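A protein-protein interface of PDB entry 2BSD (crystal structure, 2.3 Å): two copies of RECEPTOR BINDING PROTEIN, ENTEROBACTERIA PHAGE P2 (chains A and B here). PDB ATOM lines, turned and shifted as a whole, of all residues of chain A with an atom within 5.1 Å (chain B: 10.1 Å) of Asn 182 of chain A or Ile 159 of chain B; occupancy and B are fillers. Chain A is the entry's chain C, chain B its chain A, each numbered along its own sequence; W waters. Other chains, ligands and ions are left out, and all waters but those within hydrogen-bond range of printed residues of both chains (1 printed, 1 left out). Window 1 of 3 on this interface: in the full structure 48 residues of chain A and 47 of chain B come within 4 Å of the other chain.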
ATOM      1  N   ILE A 159      24.878   0.342 -16.519  1.00  0.00           N
ATOM      2  CA  ILE A 159      25.663   1.483 -16.957  1.00  0.00           C
ATOM      3  C   ILE A 159      27.120   1.053 -17.110  1.00  0.00           C
ATOM      4  O   ILE A 159      27.698   0.454 -16.197  1.00  0.00           O
ATOM      5  CB  ILE A 159      25.582   2.666 -15.970  1.00  0.00           C
ATOM      6  CG1 ILE A 159      24.139   3.022 -15.635  1.00  0.00           C
ATOM      7  CG2 ILE A 159      26.288   3.888 -16.560  1.00  0.00           C
ATOM      8  CD1 ILE A 159      24.016   4.166 -14.624  1.00  0.00           C
ATOM      9  N   VAL A 161      30.791   2.508 -17.443  1.00  0.00           N
ATOM     10  CA  VAL A 161      31.598   3.701 -17.194  1.00  0.00           C
ATOM     11  C   VAL A 161      33.068   3.383 -17.502  1.00  0.00           C
ATOM     12  O   VAL A 161      33.440   2.206 -17.529  1.00  0.00           O
ATOM     13  CB  VAL A 161      31.418   4.222 -15.735  1.00  0.00           C
ATOM     14  CG1 VAL A 161      29.964   4.589 -15.464  1.00  0.00           C
ATOM     15  CG2 VAL A 161      31.914   3.195 -14.700  1.00  0.00           C
ATOM     16  N   PRO A 162      33.901   4.399 -17.749  1.00  0.00           N
ATOM     17  CA  PRO A 162      35.325   4.152 -18.009  1.00  0.00           C
ATOM     18  C   PRO A 162      36.002   3.484 -16.813  1.00  0.00           C
ATOM     19  O   PRO A 162      35.659   3.759 -15.652  1.00  0.00           O
ATOM     20  CB  PRO A 162      35.897   5.552 -18.254  1.00  0.00           C
ATOM     21  CG  PRO A 162      34.725   6.371 -18.645  1.00  0.00           C
ATOM     22  CD  PRO A 162      33.581   5.837 -17.817  1.00  0.00           C
ATOM     23  N   LYS A 180      39.968   1.905 -10.955  1.00  0.00           N
ATOM     24  CA  LYS A 180      39.222   3.151 -10.906  1.00  0.00           C
ATOM     25  C   LYS A 180      38.078   3.140 -11.911  1.00  0.00           C
ATOM     26  O   LYS A 180      38.284   2.851 -13.095  1.00  0.00           O
ATOM     27  CB  LYS A 180      40.147   4.344 -11.170  1.00  0.00           C
ATOM     28  CG  LYS A 180      39.469   5.709 -11.057  1.00  0.00           C
ATOM     29  CD  LYS A 180      40.396   6.858 -11.468  1.00  0.00           C
ATOM     30  CE  LYS A 180      40.985   6.653 -12.871  1.00  0.00           C
ATOM     31  NZ  LYS A 180      41.383   7.943 -13.472  1.00  0.00           N
ATOM     32  N   LYS A 181      36.878   3.462 -11.425  1.00  0.00           N
ATOM     33  CA  LYS A 181      35.689   3.536 -12.264  1.00  0.00           C
ATOM     34  C   LYS A 181      35.097   4.929 -12.196  1.00  0.00           C
ATOM     35  O   LYS A 181      35.106   5.561 -11.130  1.00  0.00           O
ATOM     36  CB  LYS A 181      34.647   2.491 -11.839  1.00  0.00           C
ATOM     37  CG  LYS A 181      35.220   1.100 -11.735  1.00  0.00           C
ATOM     38  CD  LYS A 181      34.290   0.029 -12.261  1.00  0.00           C
ATOM     39  CE  LYS A 181      35.005  -1.320 -12.261  1.00  0.00           C
ATOM     40  NZ  LYS A 181      34.081  -2.454 -12.568  1.00  0.00           N
ATOM     41  N   ASN A 182      34.584   5.398 -13.338  1.00  0.00           N
ATOM     42  CA  ASN A 182      33.969   6.724 -13.468  1.00  0.00           C
ATOM     43  C   ASN A 182      34.899   7.877 -13.065  1.00  0.00           C
ATOM     44  O   ASN A 182      34.434   8.953 -12.678  1.00  0.00           O
ATOM     45  CB  ASN A 182      32.626   6.782 -12.711  1.00  0.00           C
ATOM     46  CG  ASN A 182      31.761   7.967 -13.131  1.00  0.00           C
ATOM     47  OD1 ASN A 182      31.770   8.383 -14.291  1.00  0.00           O
ATOM     48  ND2 ASN A 182      31.020   8.525 -12.180  1.00  0.00           N
ATOM     49  N   ASN A 183      36.212   7.638 -13.183  1.00  0.00           N
ATOM     50  CA  ASN A 183      37.269   8.573 -12.755  1.00  0.00           C
ATOM     51  C   ASN A 183      37.084   9.067 -11.317  1.00  0.00           C
ATOM     52  O   ASN A 183      37.373  10.228 -11.004  1.00  0.00           O
ATOM     53  CB  ASN A 183      37.428   9.753 -13.744  1.00  0.00           C
ATOM     54  CG  ASN A 183      38.765  10.518 -13.566  1.00  0.00           C
ATOM     55  OD1 ASN A 183      39.760   9.972 -13.072  1.00  0.00           O
ATOM     56  ND2 ASN A 183      38.780  11.794 -13.973  1.00  0.00           N
ATOM     57  N   ASP A 184      36.610   8.179 -10.441  1.00  0.00           N
ATOM     58  CA  ASP A 184      36.270   8.574  -9.071  1.00  0.00           C
ATOM     59  C   ASP A 184      36.387   7.474  -8.015  1.00  0.00           C
ATOM     60  O   ASP A 184      37.110   7.636  -7.031  1.00  0.00           O
ATOM     61  CB  ASP A 184      34.868   9.190  -9.012  1.00  0.00           C
ATOM     62  CG  ASP A 184      34.501   9.663  -7.611  1.00  0.00           C
ATOM     63  OD1 ASP A 184      35.393  10.175  -6.886  1.00  0.00           O
ATOM     64  OD2 ASP A 184      33.349   9.557  -7.145  1.00  0.00           O
ATOM     65  N   VAL B 150      15.833   3.814 -19.213  1.00  0.00           N
ATOM     66  CA  VAL B 150      16.743   3.281 -20.231  1.00  0.00           C
ATOM     67  C   VAL B 150      17.124   1.819 -19.942  1.00  0.00           C
ATOM     68  O   VAL B 150      17.157   1.393 -18.781  1.00  0.00           O
ATOM     69  CB  VAL B 150      18.011   4.190 -20.371  1.00  0.00           C
ATOM     70  CG1 VAL B 150      18.921   4.095 -19.147  1.00  0.00           C
ATOM     71  CG2 VAL B 150      18.797   3.877 -21.640  1.00  0.00           C
ATOM     72  N   ASP B 152      20.183   0.246 -21.343  1.00  0.00           N
ATOM     73  CA  ASP B 152      21.629   0.283 -21.126  1.00  0.00           C
ATOM     74  C   ASP B 152      22.221   1.633 -21.482  1.00  0.00           C
ATOM     75  O   ASP B 152      21.694   2.357 -22.334  1.00  0.00           O
ATOM     76  CB  ASP B 152      22.336  -0.833 -21.908  1.00  0.00           C
ATOM     77  CG  ASP B 152      21.928  -2.223 -21.440  1.00  0.00           C
ATOM     78  OD1 ASP B 152      22.387  -2.647 -20.355  1.00  0.00           O
ATOM     79  OD2 ASP B 152      21.143  -2.962 -22.078  1.00  0.00           O
ATOM     80  N   MET B 153      23.320   1.970 -20.817  1.00  0.00           N
ATOM     81  CA  MET B 153      24.033   3.210 -21.083  1.00  0.00           C
ATOM     82  C   MET B 153      25.533   2.953 -21.050  1.00  0.00           C
ATOM     83  O   MET B 153      26.033   2.225 -20.187  1.00  0.00           O
ATOM     84  CB  MET B 153      23.644   4.308 -20.075  1.00  0.00           C
ATOM     85  CG  MET B 153      24.320   5.664 -20.339  1.00  0.00           C
ATOM     86  SD  MET B 153      23.980   6.958 -19.113  1.00  0.00           S
ATOM     87  CE  MET B 153      22.672   7.714 -19.920  1.00  0.00           C
ATOM     88  N   THR B 154      26.234   3.537 -22.014  1.00  0.00           N
ATOM     89  CA  THR B 154      27.689   3.571 -22.001  1.00  0.00           C
ATOM     90  C   THR B 154      28.153   5.032 -21.991  1.00  0.00           C
ATOM     91  O   THR B 154      27.693   5.847 -22.792  1.00  0.00           O
ATOM     92  CB  THR B 154      28.284   2.739 -23.171  1.00  0.00           C
ATOM     93  OG1 THR B 154      29.692   2.985 -23.275  1.00  0.00           O
ATOM     94  CG2 THR B 154      27.753   3.207 -24.521  1.00  0.00           C
ATOM     95  N   VAL B 155      29.016   5.358 -21.036  1.00  0.00           N
ATOM     96  CA  VAL B 155      29.544   6.709 -20.854  1.00  0.00           C
ATOM     97  C   VAL B 155      31.038   6.711 -21.161  1.00  0.00           C
ATOM     98  O   VAL B 155      31.773   5.890 -20.613  1.00  0.00           O
ATOM     99  CB  VAL B 155      29.348   7.194 -19.401  1.00  0.00           C
ATOM    100  CG1 VAL B 155      29.767   8.645 -19.251  1.00  0.00           C
ATOM    101  CG2 VAL B 155      27.903   7.004 -18.964  1.00  0.00           C
ATOM    102  N   SER B 156      31.482   7.634 -22.014  1.00  0.00           N
ATOM    103  CA  SER B 156      32.890   7.720 -22.393  1.00  0.00           C
ATOM    104  C   SER B 156      33.679   8.724 -21.548  1.00  0.00           C
ATOM    105  O   SER B 156      34.893   8.611 -21.442  1.00  0.00           O
ATOM    106  CB  SER B 156      33.041   8.045 -23.887  1.00  0.00           C
ATOM    107  OG  SER B 156      32.586   9.364 -24.161  1.00  0.00           O
ATOM    108  N   GLY B 157      32.989   9.707 -20.968  1.00  0.00           N
ATOM    109  CA  GLY B 157      33.601  10.667 -20.063  1.00  0.00           C
ATOM    110  C   GLY B 157      33.289  10.302 -18.623  1.00  0.00           C
ATOM    111  O   GLY B 157      33.782   9.296 -18.115  1.00  0.00           O
ATOM    112  N   SER B 158      32.455  11.098 -17.963  1.00  0.00           N
ATOM    113  CA  SER B 158      32.122  10.850 -16.562  1.00  0.00           C
ATOM    114  C   SER B 158      30.658  11.122 -16.274  1.00  0.00           C
ATOM    115  O   SER B 158      30.026  11.941 -16.946  1.00  0.00           O
ATOM    116  CB  SER B 158      32.990  11.716 -15.640  1.00  0.00           C
ATOM    117  OG  SER B 158      34.337  11.257 -15.627  1.00  0.00           O
ATOM    118  N   ILE B 159      30.123  10.413 -15.285  1.00  0.00           N
ATOM    119  CA  ILE B 159      28.829  10.753 -14.711  1.00  0.00           C
ATOM    120  C   ILE B 159      29.052  11.533 -13.420  1.00  0.00           C
ATOM    121  O   ILE B 159      29.772  11.085 -12.524  1.00  0.00           O
ATOM    122  CB  ILE B 159      27.977   9.500 -14.425  1.00  0.00           C
ATOM    123  CG1 ILE B 159      27.910   8.591 -15.652  1.00  0.00           C
ATOM    124  CG2 ILE B 159      26.567   9.912 -13.993  1.00  0.00           C
ATOM    125  CD1 ILE B 159      27.219   7.267 -15.398  1.00  0.00           C
ATOM    126  N   ASP B 160      28.438  12.708 -13.349  1.00  0.00           N
ATOM    127  CA  ASP B 160      28.430  13.519 -12.148  1.00  0.00           C
ATOM    128  C   ASP B 160      27.119  13.280 -11.394  1.00  0.00           C
ATOM    129  O   ASP B 160      26.023  13.536 -11.907  1.00  0.00           O
ATOM    130  CB  ASP B 160      28.598  14.990 -12.517  1.00  0.00           C
ATOM    131  CG  ASP B 160      28.980  15.853 -11.328  1.00  0.00           C
ATOM    132  OD1 ASP B 160      28.103  16.581 -10.807  1.00  0.00           O
ATOM    133  OD2 ASP B 160      30.140  15.867 -10.845  1.00  0.00           O
ATOM    134  N   VAL B 161      27.238  12.749 -10.184  1.00  0.00           N
ATOM    135  CA  VAL B 161      26.086  12.473  -9.341  1.00  0.00           C
ATOM    136  C   VAL B 161      26.133  13.413  -8.137  1.00  0.00           C
ATOM    137  O   VAL B 161      27.189  13.990  -7.858  1.00  0.00           O
ATOM    138  CB  VAL B 161      26.054  10.987  -8.891  1.00  0.00           C
ATOM    139  CG1 VAL B 161      25.801  10.071 -10.095  1.00  0.00           C
ATOM    140  CG2 VAL B 161      27.349  10.592  -8.147  1.00  0.00           C
ATOM    141  N   PRO B 162      25.012  13.608  -7.444  1.00  0.00           N
ATOM    142  CA  PRO B 162      25.016  14.431  -6.226  1.00  0.00           C
ATOM    143  C   PRO B 162      25.998  13.908  -5.169  1.00  0.00           C
ATOM    144  O   PRO B 162      26.156  12.695  -5.004  1.00  0.00           O
ATOM    145  CB  PRO B 162      23.569  14.329  -5.729  1.00  0.00           C
ATOM    146  CG  PRO B 162      22.785  14.022  -6.970  1.00  0.00           C
ATOM    147  CD  PRO B 162      23.663  13.105  -7.764  1.00  0.00           C
ATOM    148  N   VAL B 163      26.664  14.839  -4.490  1.00  0.00           N
ATOM    149  CA  VAL B 163      27.641  14.520  -3.458  1.00  0.00           C
ATOM    150  C   VAL B 163      27.278  15.288  -2.199  1.00  0.00           C
ATOM    151  O   VAL B 163      27.133  16.511  -2.226  1.00  0.00           O
ATOM    152  CB  VAL B 163      29.093  14.867  -3.899  1.00  0.00           C
ATOM    153  CG1 VAL B 163      30.098  14.604  -2.766  1.00  0.00           C
ATOM    154  CG2 VAL B 163      29.494  14.082  -5.146  1.00  0.00           C
ATOM    155  N   LYS B 181      27.410   9.629  -2.165  1.00  0.00           N
ATOM    156  CA  LYS B 181      27.245   9.901  -3.591  1.00  0.00           C
ATOM    157  C   LYS B 181      26.030   9.163  -4.100  1.00  0.00           C
ATOM    158  O   LYS B 181      25.746   8.048  -3.652  1.00  0.00           O
ATOM    159  CB  LYS B 181      28.502   9.511  -4.386  1.00  0.00           C
ATOM    160  CG  LYS B 181      29.777  10.188  -3.875  1.00  0.00           C
ATOM    161  CD  LYS B 181      30.846  10.338  -4.950  1.00  0.00           C
ATOM    162  CE  LYS B 181      32.020  11.122  -4.392  1.00  0.00           C
ATOM    163  NZ  LYS B 181      33.074  11.450  -5.414  1.00  0.00           N
ATOM    164  N   ASN B 182      25.306   9.807  -5.017  1.00  0.00           N
ATOM    165  CA  ASN B 182      24.064   9.269  -5.568  1.00  0.00           C
ATOM    166  C   ASN B 182      23.050   8.930  -4.474  1.00  0.00           C
ATOM    167  O   ASN B 182      22.216   8.043  -4.643  1.00  0.00           O
ATOM    168  CB  ASN B 182      24.345   8.050  -6.461  1.00  0.00           C
ATOM    169  CG  ASN B 182      23.148   7.662  -7.323  1.00  0.00           C
ATOM    170  OD1 ASN B 182      22.432   8.524  -7.838  1.00  0.00           O
ATOM    171  ND2 ASN B 182      22.920   6.364  -7.473  1.00  0.00           N
ATOM    172  N   LEU B 185      25.786   5.429  -1.915  1.00  0.00           N
ATOM    173  CA  LEU B 185      27.086   4.926  -1.495  1.00  0.00           C
ATOM    174  C   LEU B 185      27.788   5.909  -0.561  1.00  0.00           C
ATOM    175  O   LEU B 185      27.991   7.075  -0.920  1.00  0.00           O
ATOM    176  CB  LEU B 185      27.965   4.614  -2.717  1.00  0.00           C
ATOM    177  CG  LEU B 185      29.418   4.194  -2.450  1.00  0.00           C
ATOM    178  CD1 LEU B 185      29.478   2.854  -1.711  1.00  0.00           C
ATOM    179  CD2 LEU B 185      30.222   4.144  -3.753  1.00  0.00           C
HETATM  180  O   HOH W   1      35.390   8.661 -16.128  1.00  0.00           O
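Ile 159 of chain A touches its own counterpart, Ile 159 of chain B.
Val 161 of chain A touches Ile 159 of chain B, but with the chains exchanged Ile 159 of chain A does not touch Val 161 of chain B (7.7 Å).
Asn 182 of chain A touches Ile 159 of chain B, but with the chains exchanged Ile 159 of chain A does not touch Asn 182 of chain B (7.6 Å).
Positions printed for both chains: 159, 161, 162, 181 and 182.
Of the 10 pairs that touch across the chains among the printed residues, 1 has its exchanged pair printed and touching as well.
O of Met 153 of chain B touches CA of Ile 159 of chain A, 3.3 Å away.
Ile 159 of chain B touches Ile 159 of chain A (CD1 to CG2, 3.7 Å).
Ile 159 of chain B touches Val 161 of chain A (CD1 to CG1, 3.8 Å).
Pro 162 of chain A touches Val 155 of chain B (CD to O, 3.3 Å).
Pro 162 of chain A touches Ser 156 of chain B (CG to O, 3.6 Å).
Gly 157 of chain B touches Pro 162 of chain A (O to CG, 3.1 Å).
Asn 182 of chain A touches Ser 158 of chain B (OD1 to CA, 3.4 Å).
Asn 183 of chain A touches Ser 158 of chain B (CB to OG, 3.9 Å).
Of the 16 printed residues of chain B, 7 touch a printed residue of chain A.
Along chain B the printed residues that touch a printed residue of chain A span positions 153 to 181.
Printed residues of chain A that touch a printed residue of chain B: Ile 159, Val 161, Pro 162, Asn 182, Asn 183 and Asp 184.
Hydrophobic or aromatic side chains of chain A that line the printed part of chain B: Ile 159, Val 161 and Pro 162.
Water W1 lies within hydrogen-bond range of the backbone carbonyl oxygen of Gly 157 of chain B, the side-chain hydroxyl of Ser 158 of chain B and the backbone NH of Asn 183 of chain A.
OD1 of Asn 183 of chain A lies within hydrogen-bond range of NZ of Lys 180 of chain A.
The backbone carbonyl oxygen of Pro 162 of chain A lies within hydrogen-bond range of the backbone NH of Asn 182 of chain A (3.0 Å).
The backbone NH (N) of Ile 159 of chain B lies within hydrogen-bond range of the side-chain amide oxygen (OD1) of Asn 182 of chain A (2.8 Å).
OD2 of Asp 184 of chain A is in salt-bridge range of NZ of Lys 181 of chain B, 2.6 Å away.
Of chain B, only Ser 158 (3.4 Å) and Ile 159 (2.8 Å) come within 4 Å of Asn 182 of chain A.
Pro 162 of chain A touches just these residues of chain B: Val 155 (3.3 Å), Ser 156 (3.6 Å) and Gly 157 (3.1 Å).
Asn 183 of chain A touches just one residue of chain B: Ser 158.
Of the printed residues of chain A, Lys 181 of chain B touches Asp 184.
Of the printed residues of chain A, Ser 156 of chain B touches Pro 162.
Printed residues of chain A within 4 Å of Gly 157 of chain B: Pro 162.
Of the printed residues of chain B, Asp 184 of chain A touches Lys 181 (2.6 Å).
Pro 162 of chain B touches none of the printed residues of chain A.
Thr 154 of chain B touches none of the printed residues of chain A.
The nearest printed residue of chain A that does not touch Ser 156 of chain B is Val 161 of chain A (6.2 Å).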
